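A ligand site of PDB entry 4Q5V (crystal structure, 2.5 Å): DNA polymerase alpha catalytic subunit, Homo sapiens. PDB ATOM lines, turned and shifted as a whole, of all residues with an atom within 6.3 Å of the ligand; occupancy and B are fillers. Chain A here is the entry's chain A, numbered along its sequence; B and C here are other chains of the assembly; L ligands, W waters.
N of Ser 620 sits at hydrogen-bond distance from O2 of the ligand (3.3 Å). An oxygen (O1) of the ligand sits at hydrogen-bond distance from the backbone carbonyl oxygen of Asn 619 (2.8 Å). An oxygen (O4) of the ligand lies within hydrogen-bond range of the backbone NH of Leu 529, 3.4 Å away. O4 of the ligand sits at hydrogen-bond distance from N of Tyr 530 (3.0 Å). The backbone NH (N) of Gly 623 sits at hydrogen-bond distance from an oxygen (O1) of the ligand.
The side-chain hydroxyl of Ser 620 lies within hydrogen-bond range of the backbone carbonyl oxygen of Leu 616 (3.2 Å). N2 of DG 11 of chain B sits close to O2 of DC 11 of chain C (2.7 Å). The side-chain hydroxyl (OG) of Ser 620 lies within hydrogen-bond range of N7 of DG 10 of chain B, at 2.7 Å. O of Ser 620 sits at hydrogen-bond distance from SG of Cys 624 (3.2 Å).
Merely in contact with the ligand: DG 11 of chain B (3.2 Å), Asp 669 (3.6 Å), DC 11 of chain C (3.6 Å), Tyr 622 (3.7 Å) and DG 10 of chain B (3.8 Å). Ten residues have an atom within 4 Å of the ligand: Leu 529, Tyr 530, Asn 619, Ser 620, Tyr 622, Gly 623, Asp 669, DG 10 of chain B, DG 11 of chain B and DC 11 of chain C. The nearest printed residue that does not touch the ligand is Pro 531 (4.2 Å).
Water W2 bridges O3 of the ligand (2.8 Å) and ND2 of Asn 619 (2.9 Å). Water W1 lies within hydrogen-bond range of N of Leu 529 (2.6 Å), OD1 of Asp 669 (3.0 Å), O4 of the ligand (3.1 Å) and N of Ser 528 (3.1 Å).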
ATOM      1  N   SER A 528     -20.144  -8.793 -17.079  1.00  0.00           N
ATOM      2  CA  SER A 528     -19.021  -8.360 -16.249  1.00  0.00           C
ATOM      3  C   SER A 528     -17.701  -8.564 -16.973  1.00  0.00           C
ATOM      4  O   SER A 528     -16.929  -9.473 -16.654  1.00  0.00           O
ATOM      5  CB  SER A 528     -19.025  -9.143 -14.933  1.00  0.00           C
ATOM      6  OG  SER A 528     -20.230  -8.916 -14.214  1.00  0.00           O
ATOM      7  N   LEU A 529     -17.436  -7.694 -17.950  1.00  0.00           N
ATOM      8  CA  LEU A 529     -16.206  -7.777 -18.739  1.00  0.00           C
ATOM      9  C   LEU A 529     -14.975  -7.568 -17.881  1.00  0.00           C
ATOM     10  O   LEU A 529     -14.117  -8.440 -17.785  1.00  0.00           O
ATOM     11  CB  LEU A 529     -16.217  -6.748 -19.872  1.00  0.00           C
ATOM     12  CG  LEU A 529     -15.017  -6.791 -20.831  1.00  0.00           C
ATOM     13  CD1 LEU A 529     -14.944  -8.172 -21.490  1.00  0.00           C
ATOM     14  CD2 LEU A 529     -15.156  -5.711 -21.889  1.00  0.00           C
ATOM     15  N   TYR A 530     -14.897  -6.420 -17.242  1.00  0.00           N
ATOM     16  CA  TYR A 530     -13.743  -6.127 -16.424  1.00  0.00           C
ATOM     17  C   TYR A 530     -13.428  -7.180 -15.351  1.00  0.00           C
ATOM     18  O   TYR A 530     -12.302  -7.656 -15.270  1.00  0.00           O
ATOM     19  CB  TYR A 530     -13.905  -4.734 -15.856  1.00  0.00           C
ATOM     20  CG  TYR A 530     -13.730  -3.647 -16.908  1.00  0.00           C
ATOM     21  CD1 TYR A 530     -13.511  -3.959 -18.274  1.00  0.00           C
ATOM     22  CD2 TYR A 530     -13.696  -2.301 -16.538  1.00  0.00           C
ATOM     23  CE1 TYR A 530     -13.266  -2.944 -19.220  1.00  0.00           C
ATOM     24  CE2 TYR A 530     -13.460  -1.288 -17.466  1.00  0.00           C
ATOM     25  CZ  TYR A 530     -13.248  -1.610 -18.791  1.00  0.00           C
ATOM     26  OH  TYR A 530     -13.006  -0.568 -19.645  1.00  0.00           O
ATOM     27  N   PRO A 531     -14.414  -7.569 -14.518  1.00  0.00           N
ATOM     28  CA  PRO A 531     -14.144  -8.578 -13.485  1.00  0.00           C
ATOM     29  C   PRO A 531     -13.653  -9.899 -14.101  1.00  0.00           C
ATOM     30  O   PRO A 531     -12.793 -10.583 -13.549  1.00  0.00           O
ATOM     31  CB  PRO A 531     -15.498  -8.736 -12.791  1.00  0.00           C
ATOM     32  CG  PRO A 531     -16.072  -7.394 -12.862  1.00  0.00           C
ATOM     33  CD  PRO A 531     -15.729  -6.938 -14.281  1.00  0.00           C
ATOM     34  N   LEU A 616     -21.738  -5.225  -7.091  1.00  0.00           N
ATOM     35  CA  LEU A 616     -21.143  -3.914  -6.832  1.00  0.00           C
ATOM     36  C   LEU A 616     -19.712  -4.009  -6.328  1.00  0.00           C
ATOM     37  O   LEU A 616     -18.863  -3.194  -6.668  1.00  0.00           O
ATOM     38  CB  LEU A 616     -21.967  -3.175  -5.771  1.00  0.00           C
ATOM     39  CG  LEU A 616     -23.386  -2.799  -6.188  1.00  0.00           C
ATOM     40  CD1 LEU A 616     -24.220  -2.567  -4.936  1.00  0.00           C
ATOM     41  CD2 LEU A 616     -23.355  -1.564  -7.103  1.00  0.00           C
ATOM     42  N   ALA A 618     -17.452  -6.582  -6.808  1.00  0.00           N
ATOM     43  CA  ALA A 618     -16.565  -7.017  -7.889  1.00  0.00           C
ATOM     44  C   ALA A 618     -16.236  -5.896  -8.868  1.00  0.00           C
ATOM     45  O   ALA A 618     -15.101  -5.692  -9.240  1.00  0.00           O
ATOM     46  CB  ALA A 618     -17.149  -8.209  -8.604  1.00  0.00           C
ATOM     47  N   ASN A 619     -17.248  -5.154  -9.288  1.00  0.00           N
ATOM     48  CA  ASN A 619     -16.996  -4.048 -10.207  1.00  0.00           C
ATOM     49  C   ASN A 619     -16.124  -2.923  -9.601  1.00  0.00           C
ATOM     50  O   ASN A 619     -15.266  -2.389 -10.278  1.00  0.00           O
ATOM     51  CB  ASN A 619     -18.326  -3.469 -10.699  1.00  0.00           C
ATOM     52  CG  ASN A 619     -18.933  -4.324 -11.803  1.00  0.00           C
ATOM     53  OD1 ASN A 619     -20.131  -4.237 -12.084  1.00  0.00           O
ATOM     54  ND2 ASN A 619     -18.110  -5.147 -12.432  1.00  0.00           N
ATOM     55  N   SER A 620     -16.340  -2.587  -8.344  1.00  0.00           N
ATOM     56  CA  SER A 620     -15.549  -1.525  -7.719  1.00  0.00           C
ATOM     57  C   SER A 620     -14.095  -1.910  -7.592  1.00  0.00           C
ATOM     58  O   SER A 620     -13.244  -1.056  -7.450  1.00  0.00           O
ATOM     59  CB  SER A 620     -16.097  -1.149  -6.346  1.00  0.00           C
ATOM     60  OG  SER A 620     -17.306  -0.408  -6.483  1.00  0.00           O
ATOM     61  N   MET A 621     -13.831  -3.202  -7.664  1.00  0.00           N
ATOM     62  CA  MET A 621     -12.475  -3.714  -7.547  1.00  0.00           C
ATOM     63  C   MET A 621     -11.593  -3.037  -8.591  1.00  0.00           C
ATOM     64  O   MET A 621     -10.476  -2.606  -8.308  1.00  0.00           O
ATOM     65  CB  MET A 621     -12.474  -5.219  -7.772  1.00  0.00           C
ATOM     66  CG  MET A 621     -11.325  -5.910  -7.116  1.00  0.00           C
ATOM     67  SD  MET A 621     -11.862  -6.637  -5.559  1.00  0.00           S
ATOM     68  CE  MET A 621     -12.541  -5.220  -4.689  1.00  0.00           C
ATOM     69  N   TYR A 622     -12.123  -2.964  -9.809  1.00  0.00           N
ATOM     70  CA  TYR A 622     -11.428  -2.357 -10.924  1.00  0.00           C
ATOM     71  C   TYR A 622     -11.164  -0.866 -10.700  1.00  0.00           C
ATOM     72  O   TYR A 622     -10.010  -0.428 -10.658  1.00  0.00           O
ATOM     73  CB  TYR A 622     -12.238  -2.508 -12.214  1.00  0.00           C
ATOM     74  CG  TYR A 622     -11.836  -1.493 -13.260  1.00  0.00           C
ATOM     75  CD1 TYR A 622     -10.630  -1.607 -13.918  1.00  0.00           C
ATOM     76  CD2 TYR A 622     -12.627  -0.370 -13.517  1.00  0.00           C
ATOM     77  CE1 TYR A 622     -10.198  -0.631 -14.795  1.00  0.00           C
ATOM     78  CE2 TYR A 622     -12.198   0.625 -14.403  1.00  0.00           C
ATOM     79  CZ  TYR A 622     -10.978   0.487 -15.024  1.00  0.00           C
ATOM     80  OH  TYR A 622     -10.491   1.467 -15.848  1.00  0.00           O
ATOM     81  N   GLY A 623     -12.235  -0.103 -10.558  1.00  0.00           N
ATOM     82  CA  GLY A 623     -12.086   1.329 -10.367  1.00  0.00           C
ATOM     83  C   GLY A 623     -11.130   1.729  -9.265  1.00  0.00           C
ATOM     84  O   GLY A 623     -10.567   2.822  -9.299  1.00  0.00           O
ATOM     85  N   CYS A 624     -10.934   0.871  -8.263  1.00  0.00           N
ATOM     86  CA  CYS A 624     -10.026   1.237  -7.201  1.00  0.00           C
ATOM     87  C   CYS A 624      -8.602   1.170  -7.673  1.00  0.00           C
ATOM     88  O   CYS A 624      -7.787   2.006  -7.303  1.00  0.00           O
ATOM     89  CB  CYS A 624     -10.278   0.358  -6.004  1.00  0.00           C
ATOM     90  SG  CYS A 624     -11.874   0.819  -5.277  1.00  0.00           S
ATOM     91  N   THR A 668     -17.695  -0.143 -25.130  1.00  0.00           N
ATOM     92  CA  THR A 668     -16.902  -0.840 -24.127  1.00  0.00           C
ATOM     93  C   THR A 668     -17.099  -2.353 -24.001  1.00  0.00           C
ATOM     94  O   THR A 668     -16.133  -3.102 -23.992  1.00  0.00           O
ATOM     95  CB  THR A 668     -17.150  -0.215 -22.736  1.00  0.00           C
ATOM     96  OG1 THR A 668     -16.980   1.205 -22.808  1.00  0.00           O
ATOM     97  CG2 THR A 668     -16.172  -0.774 -21.733  1.00  0.00           C
ATOM     98  N   ASP A 669     -18.347  -2.805 -23.890  1.00  0.00           N
ATOM     99  CA  ASP A 669     -18.620  -4.224 -23.702  1.00  0.00           C
ATOM    100  C   ASP A 669     -19.836  -4.730 -24.442  1.00  0.00           C
ATOM    101  O   ASP A 669     -20.293  -5.850 -24.186  1.00  0.00           O
ATOM    102  CB  ASP A 669     -18.805  -4.537 -22.216  1.00  0.00           C
ATOM    103  CG  ASP A 669     -19.991  -3.793 -21.603  1.00  0.00           C
ATOM    104  OD1 ASP A 669     -20.281  -4.019 -20.410  1.00  0.00           O
ATOM    105  OD2 ASP A 669     -20.643  -2.983 -22.292  1.00  0.00           O
ATOM    106  P    DG B  10     -14.555   7.139  -3.281  1.00  0.00           P
ATOM    107  OP1  DG B  10     -15.737   6.415  -3.805  1.00  0.00           O
ATOM    108  OP2  DG B  10     -13.925   6.689  -2.014  1.00  0.00           O
ATOM    109  O5'  DG B  10     -13.396   7.048  -4.369  1.00  0.00           O
ATOM    110  C5'  DG B  10     -13.676   7.098  -5.767  1.00  0.00           C
ATOM    111  C4'  DG B  10     -12.814   6.098  -6.501  1.00  0.00           C
ATOM    112  O4'  DG B  10     -13.252   4.767  -6.137  1.00  0.00           O
ATOM    113  C3'  DG B  10     -12.859   6.156  -8.013  1.00  0.00           C
ATOM    114  O3'  DG B  10     -11.668   6.830  -8.455  1.00  0.00           O
ATOM    115  C2'  DG B  10     -12.663   4.703  -8.425  1.00  0.00           C
ATOM    116  C1'  DG B  10     -13.197   3.894  -7.240  1.00  0.00           C
ATOM    117  N9   DG B  10     -14.550   3.359  -7.398  1.00  0.00           N
ATOM    118  C8   DG B  10     -14.980   2.088  -7.136  1.00  0.00           C
ATOM    119  N7   DG B  10     -16.268   1.957  -7.265  1.00  0.00           N
ATOM    120  C5   DG B  10     -16.711   3.206  -7.665  1.00  0.00           C
ATOM    121  C6   DG B  10     -18.030   3.697  -7.959  1.00  0.00           C
ATOM    122  O6   DG B  10     -19.110   3.092  -7.893  1.00  0.00           O
ATOM    123  N1   DG B  10     -18.017   5.031  -8.338  1.00  0.00           N
ATOM    124  C2   DG B  10     -16.888   5.816  -8.412  1.00  0.00           C
ATOM    125  N2   DG B  10     -17.073   7.082  -8.801  1.00  0.00           N
ATOM    126  N3   DG B  10     -15.664   5.384  -8.127  1.00  0.00           N
ATOM    127  C4   DG B  10     -15.655   4.079  -7.766  1.00  0.00           C
ATOM    128  P    DG B  11     -11.772   7.995  -9.574  1.00  0.00           P
ATOM    129  OP1  DG B  11     -10.651   8.968  -9.413  1.00  0.00           O
ATOM    130  OP2  DG B  11     -13.177   8.489  -9.526  1.00  0.00           O
ATOM    131  O5'  DG B  11     -11.519   7.171 -10.908  1.00  0.00           O
ATOM    132  C5'  DG B  11     -10.452   6.208 -10.975  1.00  0.00           C
ATOM    133  C4'  DG B  11     -10.477   5.501 -12.302  1.00  0.00           C
ATOM    134  O4'  DG B  11     -11.618   4.617 -12.326  1.00  0.00           O
ATOM    135  C3'  DG B  11     -10.669   6.431 -13.497  1.00  0.00           C
ATOM    136  O3'  DG B  11      -9.425   6.743 -14.139  1.00  0.00           O
ATOM    137  C2'  DG B  11     -11.418   5.552 -14.485  1.00  0.00           C
ATOM    138  C1'  DG B  11     -12.218   4.593 -13.604  1.00  0.00           C
ATOM    139  N9   DG B  11     -13.600   5.060 -13.468  1.00  0.00           N
ATOM    140  C8   DG B  11     -14.115   5.861 -12.477  1.00  0.00           C
ATOM    141  N7   DG B  11     -15.383   6.144 -12.657  1.00  0.00           N
ATOM    142  C5   DG B  11     -15.720   5.488 -13.823  1.00  0.00           C
ATOM    143  C6   DG B  11     -16.956   5.430 -14.528  1.00  0.00           C
ATOM    144  O6   DG B  11     -18.032   5.965 -14.247  1.00  0.00           O
ATOM    145  N1   DG B  11     -16.859   4.646 -15.665  1.00  0.00           N
ATOM    146  C2   DG B  11     -15.715   4.008 -16.093  1.00  0.00           C
ATOM    147  N2   DG B  11     -15.819   3.308 -17.223  1.00  0.00           N
ATOM    148  N3   DG B  11     -14.562   4.061 -15.455  1.00  0.00           N
ATOM    149  C4   DG B  11     -14.643   4.806 -14.337  1.00  0.00           C
ATOM    150  P    DC C  11     -25.370   2.663 -20.774  1.00  0.00           P
ATOM    151  OP1  DC C  11     -26.200   1.813 -21.664  1.00  0.00           O
ATOM    152  OP2  DC C  11     -25.865   2.994 -19.414  1.00  0.00           O
ATOM    153  O5'  DC C  11     -23.936   1.955 -20.665  1.00  0.00           O
ATOM    154  C5'  DC C  11     -23.344   1.367 -21.804  1.00  0.00           C
ATOM    155  C4'  DC C  11     -21.864   1.129 -21.576  1.00  0.00           C
ATOM    156  O4'  DC C  11     -21.250   2.356 -21.113  1.00  0.00           O
ATOM    157  C3'  DC C  11     -21.585   0.118 -20.471  1.00  0.00           C
ATOM    158  C2'  DC C  11     -20.231   0.554 -19.940  1.00  0.00           C
ATOM    159  C1'  DC C  11     -20.169   2.043 -20.241  1.00  0.00           C
ATOM    160  N1   DC C  11     -20.269   2.915 -19.060  1.00  0.00           N
ATOM    161  C2   DC C  11     -19.105   3.237 -18.347  1.00  0.00           C
ATOM    162  O2   DC C  11     -18.030   2.758 -18.734  1.00  0.00           O
ATOM    163  N3   DC C  11     -19.190   4.042 -17.268  1.00  0.00           N
ATOM    164  C4   DC C  11     -20.367   4.524 -16.877  1.00  0.00           C
ATOM    165  N4   DC C  11     -20.388   5.300 -15.803  1.00  0.00           N
ATOM    166  C5   DC C  11     -21.573   4.219 -17.575  1.00  0.00           C
ATOM    167  C6   DC C  11     -21.479   3.418 -18.649  1.00  0.00           C
HETATM  168  O1  LIG L   1     -15.205   0.332 -10.944  1.00  0.00           O
HETATM  169  C1  LIG L   1     -15.680   1.674 -11.100  1.00  0.00           C
HETATM  170  C2  LIG L   1     -17.073   1.666 -11.744  1.00  0.00           C
HETATM  171  C3  LIG L   1     -17.505   3.119 -11.931  1.00  0.00           C
HETATM  172  C4  LIG L   1     -18.041   0.958 -10.806  1.00  0.00           C
HETATM  173  O2  LIG L   1     -17.554  -0.358 -10.516  1.00  0.00           O
HETATM  174  C5  LIG L   1     -19.420   0.869 -11.453  1.00  0.00           C
HETATM  175  C6  LIG L   1     -19.311   0.017 -12.707  1.00  0.00           C
HETATM  176  C7  LIG L   1     -18.371   0.688 -13.698  1.00  0.00           C
HETATM  177  C8  LIG L   1     -18.991   2.012 -14.169  1.00  0.00           C
HETATM  178  C9  LIG L   1     -17.005   0.921 -13.073  1.00  0.00           C
HETATM  179  C10 LIG L   1     -16.053   1.598 -14.046  1.00  0.00           C
HETATM  180  C11 LIG L   1     -15.888   0.747 -15.293  1.00  0.00           C
HETATM  181  C12 LIG L   1     -17.263   0.502 -15.891  1.00  0.00           C
HETATM  182  C13 LIG L   1     -17.305  -0.387 -17.113  1.00  0.00           C
HETATM  183  C14 LIG L   1     -18.651  -1.091 -16.982  1.00  0.00           C
HETATM  184  C15 LIG L   1     -19.351  -0.414 -15.809  1.00  0.00           C
HETATM  185  C16 LIG L   1     -18.158  -0.227 -14.894  1.00  0.00           C
HETATM  186  C17 LIG L   1     -17.586  -1.561 -14.438  1.00  0.00           C
HETATM  187  C18 LIG L   1     -17.277  -2.539 -15.558  1.00  0.00           C
HETATM  188  C19 LIG L   1     -18.386  -2.543 -16.610  1.00  0.00           C
HETATM  189  O3  LIG L   1     -19.567  -3.140 -16.074  1.00  0.00           O
HETATM  190  C20 LIG L   1     -17.897  -3.328 -17.827  1.00  0.00           C
HETATM  191  O4  LIG L   1     -17.013  -4.368 -17.388  1.00  0.00           O
HETATM  192  O   HOH W   1     -19.435  -6.017 -18.377  1.00  0.00           O
HETATM  193  O   HOH W   2     -19.045  -5.726 -15.111  1.00  0.00           O
